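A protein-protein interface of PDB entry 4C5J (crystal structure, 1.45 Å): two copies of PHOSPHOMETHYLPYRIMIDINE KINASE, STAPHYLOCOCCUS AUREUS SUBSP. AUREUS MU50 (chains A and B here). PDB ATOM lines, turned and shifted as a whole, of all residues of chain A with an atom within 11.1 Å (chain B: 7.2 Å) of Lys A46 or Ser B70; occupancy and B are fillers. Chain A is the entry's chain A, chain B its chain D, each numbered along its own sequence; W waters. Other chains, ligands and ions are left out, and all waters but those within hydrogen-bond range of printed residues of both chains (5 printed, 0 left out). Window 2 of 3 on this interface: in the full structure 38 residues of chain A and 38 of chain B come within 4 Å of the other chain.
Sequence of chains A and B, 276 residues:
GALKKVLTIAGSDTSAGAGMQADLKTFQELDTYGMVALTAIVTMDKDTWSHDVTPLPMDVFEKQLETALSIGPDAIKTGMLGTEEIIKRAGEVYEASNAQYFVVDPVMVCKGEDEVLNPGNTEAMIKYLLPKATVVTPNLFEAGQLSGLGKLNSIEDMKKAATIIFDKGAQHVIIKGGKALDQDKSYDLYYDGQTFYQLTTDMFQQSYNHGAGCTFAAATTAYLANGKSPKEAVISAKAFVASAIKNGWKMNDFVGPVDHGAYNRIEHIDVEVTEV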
ATOM      1  N   THR A  14     -17.955 -12.704   9.578  1.00  0.00           N
ATOM      2  CA  THR A  14     -16.910 -13.686   9.805  1.00  0.00           C
ATOM      3  C   THR A  14     -17.249 -15.016   9.074  1.00  0.00           C
ATOM      4  O   THR A  14     -16.349 -15.733   8.610  1.00  0.00           O
ATOM      5  CB  THR A  14     -16.631 -13.952  11.311  1.00  0.00           C
ATOM      6  OG1 THR A  14     -16.285 -12.740  11.933  1.00  0.00           O
ATOM      7  CG2 THR A  14     -15.499 -14.936  11.464  1.00  0.00           C
ATOM      8  N   SER A  15     -18.523 -15.320   8.897  1.00  0.00           N
ATOM      9  CA  SER A  15     -18.944 -16.502   8.181  1.00  0.00           C
ATOM     10  C   SER A  15     -18.618 -16.473   6.637  1.00  0.00           C
ATOM     11  O   SER A  15     -18.627 -17.552   6.017  1.00  0.00           O
ATOM     12  CB  SER A  15     -20.422 -16.874   8.377  1.00  0.00           C
ATOM     13  OG  SER A  15     -21.309 -15.939   7.707  1.00  0.00           O
ATOM     14  N   VAL A  42     -18.613  -8.785  12.618  1.00  0.00           N
ATOM     15  CA  VAL A  42     -19.709  -9.585  13.048  1.00  0.00           C
ATOM     16  C   VAL A  42     -19.260 -11.026  13.271  1.00  0.00           C
ATOM     17  O   VAL A  42     -18.730 -11.675  12.343  1.00  0.00           O
ATOM     18  CB  VAL A  42     -20.892  -9.541  12.056  1.00  0.00           C
ATOM     19  CG1 VAL A  42     -22.080 -10.314  12.591  1.00  0.00           C
ATOM     20  CG2 VAL A  42     -21.249  -8.121  11.707  1.00  0.00           C
ATOM     21  N   THR A  43     -19.454 -11.505  14.489  1.00  0.00           N
ATOM     22  CA  THR A  43     -19.156 -12.887  14.795  1.00  0.00           C
ATOM     23  C   THR A  43     -20.417 -13.630  15.269  1.00  0.00           C
ATOM     24  O   THR A  43     -21.464 -13.010  15.527  1.00  0.00           O
ATOM     25  CB  THR A  43     -18.041 -12.932  15.864  1.00  0.00           C
ATOM     26  OG1 THR A  43     -18.495 -12.280  17.043  1.00  0.00           O
ATOM     27  CG2 THR A  43     -16.766 -12.296  15.364  1.00  0.00           C
ATOM     28  N   MET A  44     -20.343 -14.973  15.309  1.00  0.00           N
ATOM     29  CA  MET A  44     -21.450 -15.830  15.647  1.00  0.00           C
ATOM     30  C   MET A  44     -21.082 -16.885  16.690  1.00  0.00           C
ATOM     31  O   MET A  44     -20.032 -17.520  16.604  1.00  0.00           O
ATOM     32  CB  MET A  44     -21.962 -16.532  14.360  1.00  0.00           C
ATOM     33  CG  MET A  44     -22.489 -15.540  13.335  1.00  0.00           C
ATOM     34  SD  MET A  44     -21.154 -14.925  12.247  1.00  0.00           S
ATOM     35  CE  MET A  44     -22.056 -13.851  11.198  1.00  0.00           C
ATOM     36  N   ASP A  45     -21.999 -17.100  17.656  1.00  0.00           N
ATOM     37  CA  ASP A  45     -21.838 -18.100  18.697  1.00  0.00           C
ATOM     38  C   ASP A  45     -21.835 -19.506  18.054  1.00  0.00           C
ATOM     39  O   ASP A  45     -22.722 -19.801  17.225  1.00  0.00           O
ATOM     40  CB  ASP A  45     -23.029 -18.078  19.744  1.00  0.00           C
ATOM     41  CG  ASP A  45     -22.829 -19.039  20.926  1.00  0.00           C
ATOM     42  OD1 ASP A  45     -22.255 -18.605  21.939  1.00  0.00           O
ATOM     43  OD2 ASP A  45     -23.283 -20.206  20.836  1.00  0.00           O
ATOM     44  N   LYS A  46     -20.903 -20.377  18.438  1.00  0.00           N
ATOM     45  CA  LYS A  46     -20.810 -21.720  17.853  1.00  0.00           C
ATOM     46  C   LYS A  46     -22.036 -22.640  18.023  1.00  0.00           C
ATOM     47  O   LYS A  46     -22.231 -23.589  17.220  1.00  0.00           O
ATOM     48  CB  LYS A  46     -19.543 -22.431  18.360  1.00  0.00           C
ATOM     49  CG  LYS A  46     -19.567 -22.673  19.872  1.00  0.00           C
ATOM     50  CD  LYS A  46     -18.412 -23.503  20.416  1.00  0.00           C
ATOM     51  CE  LYS A  46     -18.695 -24.004  21.871  1.00  0.00           C
ATOM     52  NZ  LYS A  46     -17.642 -24.942  22.283  1.00  0.00           N
ATOM     53  N   ASP A  47     -22.840 -22.361  19.072  1.00  0.00           N
ATOM     54  CA  ASP A  47     -23.941 -23.236  19.499  1.00  0.00           C
ATOM     55  C   ASP A  47     -25.305 -22.740  19.000  1.00  0.00           C
ATOM     56  O   ASP A  47     -26.090 -23.534  18.447  1.00  0.00           O
ATOM     57  CB  ASP A  47     -23.898 -23.390  21.022  1.00  0.00           C
ATOM     58  CG  ASP A  47     -22.658 -24.140  21.482  1.00  0.00           C
ATOM     59  OD1 ASP A  47     -22.324 -25.179  20.845  1.00  0.00           O
ATOM     60  OD2 ASP A  47     -22.016 -23.705  22.461  1.00  0.00           O
ATOM     61  N   THR A  48     -25.543 -21.432  19.170  1.00  0.00           N
ATOM     62  CA  THR A  48     -26.820 -20.792  18.845  1.00  0.00           C
ATOM     63  C   THR A  48     -26.755 -19.917  17.550  1.00  0.00           C
ATOM     64  O   THR A  48     -27.784 -19.525  16.991  1.00  0.00           O
ATOM     65  CB  THR A  48     -27.280 -19.891  20.019  1.00  0.00           C
ATOM     66  OG1 THR A  48     -26.401 -18.774  20.123  1.00  0.00           O
ATOM     67  CG2 THR A  48     -27.276 -20.650  21.388  1.00  0.00           C
ATOM     68  N   TRP A  49     -25.525 -19.608  17.085  1.00  0.00           N
ATOM     69  CA  TRP A  49     -25.302 -18.732  15.954  1.00  0.00           C
ATOM     70  C   TRP A  49     -25.755 -17.291  16.205  1.00  0.00           C
ATOM     71  O   TRP A  49     -25.981 -16.516  15.278  1.00  0.00           O
ATOM     72  CB  TRP A  49     -25.885 -19.350  14.686  1.00  0.00           C
ATOM     73  CG  TRP A  49     -25.081 -19.013  13.459  1.00  0.00           C
ATOM     74  CD1 TRP A  49     -25.426 -18.184  12.394  1.00  0.00           C
ATOM     75  CD2 TRP A  49     -23.736 -19.440  13.214  1.00  0.00           C
ATOM     76  NE1 TRP A  49     -24.370 -18.141  11.484  1.00  0.00           N
ATOM     77  CE2 TRP A  49     -23.329 -18.891  11.987  1.00  0.00           C
ATOM     78  CE3 TRP A  49     -22.834 -20.234  13.929  1.00  0.00           C
ATOM     79  CZ2 TRP A  49     -22.080 -19.127  11.481  1.00  0.00           C
ATOM     80  CZ3 TRP A  49     -21.623 -20.500  13.392  1.00  0.00           C
ATOM     81  CH2 TRP A  49     -21.244 -19.949  12.192  1.00  0.00           C
ATOM     82  N   SER A  50     -25.952 -16.986  17.496  1.00  0.00           N
ATOM     83  CA  SER A  50     -26.310 -15.643  17.902  1.00  0.00           C
ATOM     84  C   SER A  50     -25.206 -14.731  17.405  1.00  0.00           C
ATOM     85  O   SER A  50     -24.013 -15.036  17.580  1.00  0.00           O
ATOM     86  CB  SER A  50     -26.402 -15.523  19.432  1.00  0.00           C
ATOM     87  OG  SER A  50     -26.736 -14.203  19.763  1.00  0.00           O
ATOM     88  N   HIS A  51     -25.596 -13.607  16.811  1.00  0.00           N
ATOM     89  CA  HIS A  51     -24.642 -12.623  16.326  1.00  0.00           C
ATOM     90  C   HIS A  51     -24.157 -11.598  17.370  1.00  0.00           C
ATOM     91  O   HIS A  51     -24.903 -11.222  18.273  1.00  0.00           O
ATOM     92  CB  HIS A  51     -25.260 -11.805  15.232  1.00  0.00           C
ATOM     93  CG  HIS A  51     -25.454 -12.511  13.951  1.00  0.00           C
ATOM     94  ND1 HIS A  51     -25.776 -13.856  13.864  1.00  0.00           N
ATOM     95  CD2 HIS A  51     -25.455 -12.037  12.689  1.00  0.00           C
ATOM     96  CE1 HIS A  51     -25.925 -14.184  12.586  1.00  0.00           C
ATOM     97  NE2 HIS A  51     -25.727 -13.103  11.856  1.00  0.00           N
ATOM     98  N   ASP A  52     -22.898 -11.192  17.219  1.00  0.00           N
ATOM     99  CA  ASP A  52     -22.268 -10.159  18.017  1.00  0.00           C
ATOM    100  C   ASP A  52     -21.575  -9.208  17.062  1.00  0.00           C
ATOM    101  O   ASP A  52     -20.680  -9.563  16.313  1.00  0.00           O
ATOM    102  CB  ASP A  52     -21.249 -10.779  18.959  1.00  0.00           C
ATOM    103  CG  ASP A  52     -20.676  -9.820  19.906  1.00  0.00           C
ATOM    104  OD1 ASP A  52     -21.173  -8.708  20.009  1.00  0.00           O
ATOM    105  OD2 ASP A  52     -19.702 -10.176  20.582  1.00  0.00           O
ATOM    106  N   TRP A 249     -25.114 -23.159  -0.682  1.00  0.00           N
ATOM    107  CA  TRP A 249     -24.816 -24.413  -0.004  1.00  0.00           C
ATOM    108  C   TRP A 249     -24.989 -24.287   1.519  1.00  0.00           C
ATOM    109  O   TRP A 249     -24.914 -23.207   2.065  1.00  0.00           O
ATOM    110  CB  TRP A 249     -23.417 -24.958  -0.373  1.00  0.00           C
ATOM    111  CG  TRP A 249     -22.299 -23.985  -0.070  1.00  0.00           C
ATOM    112  CD1 TRP A 249     -21.840 -22.939  -0.887  1.00  0.00           C
ATOM    113  CD2 TRP A 249     -21.462 -23.965   1.085  1.00  0.00           C
ATOM    114  NE1 TRP A 249     -20.844 -22.309  -0.299  1.00  0.00           N
ATOM    115  CE2 TRP A 249     -20.582 -22.864   0.934  1.00  0.00           C
ATOM    116  CE3 TRP A 249     -21.399 -24.717   2.298  1.00  0.00           C
ATOM    117  CZ2 TRP A 249     -19.620 -22.554   1.900  1.00  0.00           C
ATOM    118  CZ3 TRP A 249     -20.480 -24.382   3.222  1.00  0.00           C
ATOM    119  CH2 TRP A 249     -19.582 -23.315   3.031  1.00  0.00           C
ATOM    120  N   LYS A 250     -25.244 -25.420   2.185  1.00  0.00           N
ATOM    121  CA  LYS A 250     -25.559 -25.429   3.611  1.00  0.00           C
ATOM    122  C   LYS A 250     -24.235 -25.379   4.412  1.00  0.00           C
ATOM    123  O   LYS A 250     -23.419 -26.316   4.378  1.00  0.00           O
ATOM    124  CB  LYS A 250     -26.303 -26.730   3.980  1.00  0.00           C
ATOM    125  CG  LYS A 250     -26.732 -26.764   5.433  1.00  0.00           C
ATOM    126  CD  LYS A 250     -27.569 -28.019   5.671  1.00  0.00           C
ATOM    127  CE  LYS A 250     -28.041 -28.036   7.113  1.00  0.00           C
ATOM    128  NZ  LYS A 250     -28.963 -29.161   7.467  1.00  0.00           N
ATOM    129  N   MET A 251     -24.056 -24.335   5.185  1.00  0.00           N
ATOM    130  CA  MET A 251     -22.878 -24.224   6.030  1.00  0.00           C
ATOM    131  C   MET A 251     -23.048 -24.869   7.387  1.00  0.00           C
ATOM    132  O   MET A 251     -22.105 -25.471   7.920  1.00  0.00           O
ATOM    133  CB  MET A 251     -22.522 -22.740   6.161  1.00  0.00           C
ATOM    134  CG  MET A 251     -21.504 -22.332   7.224  1.00  0.00           C
ATOM    135  SD  MET A 251     -21.003 -20.649   7.148  1.00  0.00           S
ATOM    136  CE  MET A 251     -19.994 -20.691   5.728  1.00  0.00           C
ATOM    137  N   ASN A 252     -24.227 -24.657   7.965  1.00  0.00           N
ATOM    138  CA  ASN A 252     -24.602 -25.254   9.222  1.00  0.00           C
ATOM    139  C   ASN A 252     -26.116 -25.232   9.316  1.00  0.00           C
ATOM    140  O   ASN A 252     -26.774 -24.925   8.313  1.00  0.00           O
ATOM    141  CB  ASN A 252     -23.889 -24.616  10.407  1.00  0.00           C
ATOM    142  CG  ASN A 252     -24.213 -23.149  10.563  1.00  0.00           C
ATOM    143  OD1 ASN A 252     -25.287 -22.705  10.186  1.00  0.00           O
ATOM    144  ND2 ASN A 252     -23.278 -22.387  11.090  1.00  0.00           N
ATOM    145  N   ASP A 253     -26.670 -25.568  10.486  1.00  0.00           N
ATOM    146  CA  ASP A 253     -28.113 -25.621  10.644  1.00  0.00           C
ATOM    147  C   ASP A 253     -28.807 -24.234  10.565  1.00  0.00           C
ATOM    148  O   ASP A 253     -30.021 -24.148  10.432  1.00  0.00           O
ATOM    149  CB  ASP A 253     -28.473 -26.257  11.983  1.00  0.00           C
ATOM    150  CG  ASP A 253     -28.159 -27.785  12.029  1.00  0.00           C
ATOM    151  OD1 ASP A 253     -28.378 -28.521  11.043  1.00  0.00           O
ATOM    152  OD2 ASP A 253     -27.732 -28.193  13.094  1.00  0.00           O
ATOM    153  N   PHE A 254     -28.034 -23.162  10.598  1.00  0.00           N
ATOM    154  CA  PHE A 254     -28.516 -21.835  10.698  1.00  0.00           C
ATOM    155  C   PHE A 254     -28.368 -20.999   9.438  1.00  0.00           C
ATOM    156  O   PHE A 254     -29.081 -20.003   9.304  1.00  0.00           O
ATOM    157  CB  PHE A 254     -27.694 -21.123  11.789  1.00  0.00           C
ATOM    158  CG  PHE A 254     -27.719 -21.782  13.118  1.00  0.00           C
ATOM    159  CD1 PHE A 254     -28.831 -21.627  13.911  1.00  0.00           C
ATOM    160  CD2 PHE A 254     -26.637 -22.551  13.574  1.00  0.00           C
ATOM    161  CE1 PHE A 254     -28.899 -22.165  15.177  1.00  0.00           C
ATOM    162  CE2 PHE A 254     -26.690 -23.106  14.850  1.00  0.00           C
ATOM    163  CZ  PHE A 254     -27.846 -22.932  15.651  1.00  0.00           C
ATOM    164  N   VAL A 255     -27.434 -21.332   8.554  1.00  0.00           N
ATOM    165  CA  VAL A 255     -27.089 -20.434   7.442  1.00  0.00           C
ATOM    166  C   VAL A 255     -26.532 -21.266   6.264  1.00  0.00           C
ATOM    167  O   VAL A 255     -25.897 -22.365   6.454  1.00  0.00           O
ATOM    168  CB  VAL A 255     -26.104 -19.327   7.946  1.00  0.00           C
ATOM    169  CG1 VAL A 255     -24.680 -19.813   8.254  1.00  0.00           C
ATOM    170  CG2 VAL A 255     -26.008 -18.156   6.993  1.00  0.00           C
ATOM    171  N   LYS B   5     -13.250 -24.997   2.221  1.00  0.00           N
ATOM    172  CA  LYS B   5     -13.280 -23.855   3.086  1.00  0.00           C
ATOM    173  C   LYS B   5     -11.855 -23.560   3.499  1.00  0.00           C
ATOM    174  O   LYS B   5     -11.192 -24.347   4.140  1.00  0.00           O
ATOM    175  CB  LYS B   5     -14.166 -24.150   4.332  1.00  0.00           C
ATOM    176  CG  LYS B   5     -15.638 -24.337   3.961  1.00  0.00           C
ATOM    177  CD  LYS B   5     -16.427 -24.973   5.079  1.00  0.00           C
ATOM    178  CE  LYS B   5     -16.225 -26.475   5.145  1.00  0.00           C
ATOM    179  NZ  LYS B   5     -16.793 -27.036   6.397  1.00  0.00           N
ATOM    180  N   MET B  35     -12.239 -17.430   3.829  1.00  0.00           N
ATOM    181  CA  MET B  35     -12.651 -16.933   5.121  1.00  0.00           C
ATOM    182  C   MET B  35     -11.476 -16.231   5.771  1.00  0.00           C
ATOM    183  O   MET B  35     -10.321 -16.607   5.491  1.00  0.00           O
ATOM    184  CB  MET B  35     -13.062 -18.150   6.010  1.00  0.00           C
ATOM    185  CG  MET B  35     -14.109 -19.039   5.375  1.00  0.00           C
ATOM    186  SD  MET B  35     -14.410 -20.523   6.301  1.00  0.00           S
ATOM    187  CE  MET B  35     -14.713 -19.816   7.918  1.00  0.00           C
ATOM    188  N   GLN B  64     -13.847 -14.305  16.450  1.00  0.00           N
ATOM    189  CA  GLN B  64     -13.757 -14.661  15.012  1.00  0.00           C
ATOM    190  C   GLN B  64     -13.256 -16.089  14.874  1.00  0.00           C
ATOM    191  O   GLN B  64     -13.773 -16.880  14.077  1.00  0.00           O
ATOM    192  CB  GLN B  64     -12.827 -13.727  14.306  1.00  0.00           C
ATOM    193  CG  GLN B  64     -13.361 -12.291  14.120  1.00  0.00           C
ATOM    194  CD  GLN B  64     -12.306 -11.461  13.506  1.00  0.00           C
ATOM    195  OE1 GLN B  64     -12.180 -11.415  12.261  1.00  0.00           O
ATOM    196  NE2 GLN B  64     -11.421 -10.920  14.330  1.00  0.00           N
ATOM    197  N   LEU B  65     -12.252 -16.448  15.674  1.00  0.00           N
ATOM    198  CA  LEU B  65     -11.760 -17.811  15.625  1.00  0.00           C
ATOM    199  C   LEU B  65     -12.839 -18.861  16.018  1.00  0.00           C
ATOM    200  O   LEU B  65     -12.895 -19.930  15.440  1.00  0.00           O
ATOM    201  CB  LEU B  65     -10.561 -18.001  16.558  1.00  0.00           C
ATOM    202  CG  LEU B  65      -9.289 -17.236  16.199  1.00  0.00           C
ATOM    203  CD1 LEU B  65      -8.227 -17.516  17.283  1.00  0.00           C
ATOM    204  CD2 LEU B  65      -8.739 -17.636  14.845  1.00  0.00           C
ATOM    205  N   GLU B  66     -13.648 -18.548  17.048  1.00  0.00           N
ATOM    206  CA  GLU B  66     -14.735 -19.428  17.408  1.00  0.00           C
ATOM    207  C   GLU B  66     -15.675 -19.708  16.237  1.00  0.00           C
ATOM    208  O   GLU B  66     -16.062 -20.798  15.975  1.00  0.00           O
ATOM    209  CB  GLU B  66     -15.520 -18.881  18.618  1.00  0.00           C
ATOM    210  CG  GLU B  66     -16.793 -19.707  18.887  1.00  0.00           C
ATOM    211  CD  GLU B  66     -17.605 -19.268  20.129  1.00  0.00           C
ATOM    212  OE1 GLU B  66     -16.975 -18.800  21.130  1.00  0.00           O
ATOM    213  OE2 GLU B  66     -18.863 -19.359  20.123  1.00  0.00           O
ATOM    214  N   THR B  67     -16.059 -18.657  15.567  1.00  0.00           N
ATOM    215  CA  THR B  67     -16.897 -18.743  14.405  1.00  0.00           C
ATOM    216  C   THR B  67     -16.244 -19.565  13.281  1.00  0.00           C
ATOM    217  O   THR B  67     -16.837 -20.521  12.783  1.00  0.00           O
ATOM    218  CB  THR B  67     -17.292 -17.364  13.932  1.00  0.00           C
ATOM    219  OG1 THR B  67     -18.025 -16.687  14.971  1.00  0.00           O
ATOM    220  CG2 THR B  67     -18.175 -17.462  12.710  1.00  0.00           C
ATOM    221  N   ALA B  68     -15.001 -19.236  12.954  1.00  0.00           N
ATOM    222  CA  ALA B  68     -14.319 -19.933  11.848  1.00  0.00           C
ATOM    223  C   ALA B  68     -14.157 -21.420  12.190  1.00  0.00           C
ATOM    224  O   ALA B  68     -14.328 -22.252  11.328  1.00  0.00           O
ATOM    225  CB  ALA B  68     -12.970 -19.291  11.620  1.00  0.00           C
ATOM    226  N   LEU B  69     -13.814 -21.744  13.454  1.00  0.00           N
ATOM    227  CA  LEU B  69     -13.575 -23.123  13.816  1.00  0.00           C
ATOM    228  C   LEU B  69     -14.897 -23.898  13.763  1.00  0.00           C
ATOM    229  O   LEU B  69     -14.911 -25.069  13.399  1.00  0.00           O
ATOM    230  CB  LEU B  69     -13.014 -23.184  15.248  1.00  0.00           C
ATOM    231  CG  LEU B  69     -12.603 -24.552  15.756  1.00  0.00           C
ATOM    232  CD1 LEU B  69     -11.282 -24.964  15.069  1.00  0.00           C
ATOM    233  CD2 LEU B  69     -12.440 -24.527  17.285  1.00  0.00           C
ATOM    234  N   SER B  70     -15.999 -23.280  14.181  1.00  0.00           N
ATOM    235  CA  SER B  70     -17.314 -23.905  14.082  1.00  0.00           C
ATOM    236  C   SER B  70     -17.645 -24.263  12.636  1.00  0.00           C
ATOM    237  O   SER B  70     -18.164 -25.305  12.347  1.00  0.00           O
ATOM    238  CB  SER B  70     -18.375 -22.945  14.668  1.00  0.00           C
ATOM    239  OG  SER B  70     -19.683 -23.500  14.650  1.00  0.00           O
ATOM    240  N   ILE B  71     -17.372 -23.358  11.719  1.00  0.00           N
ATOM    241  CA  ILE B  71     -17.656 -23.609  10.289  1.00  0.00           C
ATOM    242  C   ILE B  71     -16.822 -24.778   9.751  1.00  0.00           C
ATOM    243  O   ILE B  71     -17.301 -25.589   8.974  1.00  0.00           O
ATOM    244  CB  ILE B  71     -17.383 -22.312   9.471  1.00  0.00           C
ATOM    245  CG1 ILE B  71     -18.460 -21.311   9.788  1.00  0.00           C
ATOM    246  CG2 ILE B  71     -17.428 -22.606   7.999  1.00  0.00           C
ATOM    247  CD1 ILE B  71     -18.163 -19.871   9.441  1.00  0.00           C
ATOM    248  N   GLY B  72     -15.582 -24.848  10.245  1.00  0.00           N
ATOM    249  CA  GLY B  72     -14.755 -26.007   9.975  1.00  0.00           C
ATOM    250  C   GLY B  72     -13.920 -25.821   8.700  1.00  0.00           C
ATOM    251  O   GLY B  72     -14.281 -26.290   7.645  1.00  0.00           O
ATOM    252  N   PRO B  73     -12.757 -25.175   8.823  1.00  0.00           N
ATOM    253  CA  PRO B  73     -11.934 -25.043   7.625  1.00  0.00           C
ATOM    254  C   PRO B  73     -11.297 -26.334   7.177  1.00  0.00           C
ATOM    255  O   PRO B  73     -10.919 -27.145   7.996  1.00  0.00           O
ATOM    256  CB  PRO B  73     -10.856 -24.051   8.048  1.00  0.00           C
ATOM    257  CG  PRO B  73     -10.793 -24.100   9.514  1.00  0.00           C
ATOM    258  CD  PRO B  73     -12.124 -24.581  10.010  1.00  0.00           C
HETATM  259  O   HOH W   1     -19.554 -25.568  16.496  1.00  0.00           O
HETATM  260  O   HOH W   2     -21.237 -24.014  12.511  1.00  0.00           O
HETATM  261  O   HOH W   3     -14.411 -11.315  10.574  1.00  0.00           O
HETATM  262  O   HOH W   4     -17.926 -16.213  18.245  1.00  0.00           O
HETATM  263  O   HOH W   5     -19.609 -25.679   6.726  1.00  0.00           O
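O of Met A44 sits at hydrogen-bond distance from OG1 of Thr B67 (2.7 Å).
The backbone NH of Lys A46 sits at hydrogen-bond distance from the side-chain carboxylate of Glu B66 (2.8 Å).
The backbone carbonyl oxygen (O) of Val A42 is in hydrogen-bond range of the side-chain hydroxyl (OG1) of Thr A14, 2.7 Å away.
The backbone NH of Asp A52 is in hydrogen-bond range of the backbone carbonyl oxygen of Thr A43.
The backbone NH (N) of Asp A47 sits at hydrogen-bond distance from the side-chain carboxylate (OD2) of Asp A45 (2.8 Å).
The side-chain carboxylate of Asp A45 lies within hydrogen-bond range of the backbone NH of Thr A48, at 3.1 Å.
The backbone carbonyl oxygen (O) of Trp A49 sits at hydrogen-bond distance from a ring nitrogen (ND1) of His A51 (3.0 Å).
The side-chain amino group (NZ) of Lys B5 is in hydrogen-bond range of the backbone carbonyl oxygen (O) of Ile B71, at 3.0 Å.
Among the printed residues, pairs that only touch across the chains: Thr A14 with Gln B64 (3.7 Å), Thr A14 with Thr B67 (3.9 Å), Ser A15 with Ile B71 (3.7 Å), Thr A43 with Gln B64 (3.6 Å), Thr A43 with Thr B67 (3.9 Å), Asp A45 with Glu B66 (3.5 Å), Lys A46 with Ser B70 (3.6 Å), Trp A49 with Thr B67 (3.98 Å), Trp A49 with Ser B70 (3.8 Å), Trp A49 with Ile B71 (3.9 Å) and Met A251 with Ile B71 (3.7 Å).
Printed residues of chain B within 4 Å of Lys A46: Glu B66 and Ser B70.
Ser B70 touches just these residues of chain A: Lys A46 (3.6 Å) and Trp A49 (3.8 Å).
Glu B66 touches just these residues of chain A: Asp A45 and Lys A46.
No residue of chain A comes within 4 Å of Ala B68.
Leu B69 touches none of the printed residues of chain A.
Ile B71 touches just these residues of chain A: Ser A15 (3.7 Å), Trp A49 (3.9 Å) and Met A251 (3.7 Å).
Printed residues of chain B within 4 Å of Met A44: Thr B67.
Of the printed residues of chain A, Gln B64 touches Thr A14 (3.7 Å) and Thr A43 (3.6 Å).
The nearest residue of chain B that does not touch Lys A46 is Thr B67 (5.8 Å).
The nearest printed residue of chain B that does not touch Met A251 is Lys B5 (5.6 Å).
Of the 12 printed residues of chain B, 5 touch a printed residue of chain A.
Hydrophobic or aromatic side chains of chain B that line the printed part of chain A: Ile B71.
Along chain A the printed residues that touch a printed residue of chain B span positions 14 to 251.
Among the printed residues, 13 pairs touch across the chains.
Among the printed residues, no Asp or Glu carboxylate lies within 4 Å of a Lys or Arg side-chain nitrogen of the other chain.
No position is printed for both chains.
Of the 13 pairs that touch across the chains among the printed residues, none has its exchanged pair printed and touching as well.
Water W2 lies within hydrogen-bond range of the side-chain hydroxyl (OG) of Ser B70 (2.7 Å) and the side-chain amide nitrogen (ND2) of Asn A252 (3.0 Å).
Water W3 lies within hydrogen-bond range of the side-chain hydroxyl of Thr A14 (2.7 Å) and the side-chain amide oxygen of Gln B64 (2.8 Å).
Water W5 lies within hydrogen-bond range of O of Met A251, NZ of Lys B5 and O of Ile B71.
Water W1 bridges the side-chain hydroxyl of Ser B70 (2.8 Å) and the backbone carbonyl oxygen of Lys A46 (3.4 Å).
Water W4 bridges O of Met A44 (3.0 Å) and OG1 of Thr B67 (3.3 Å).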
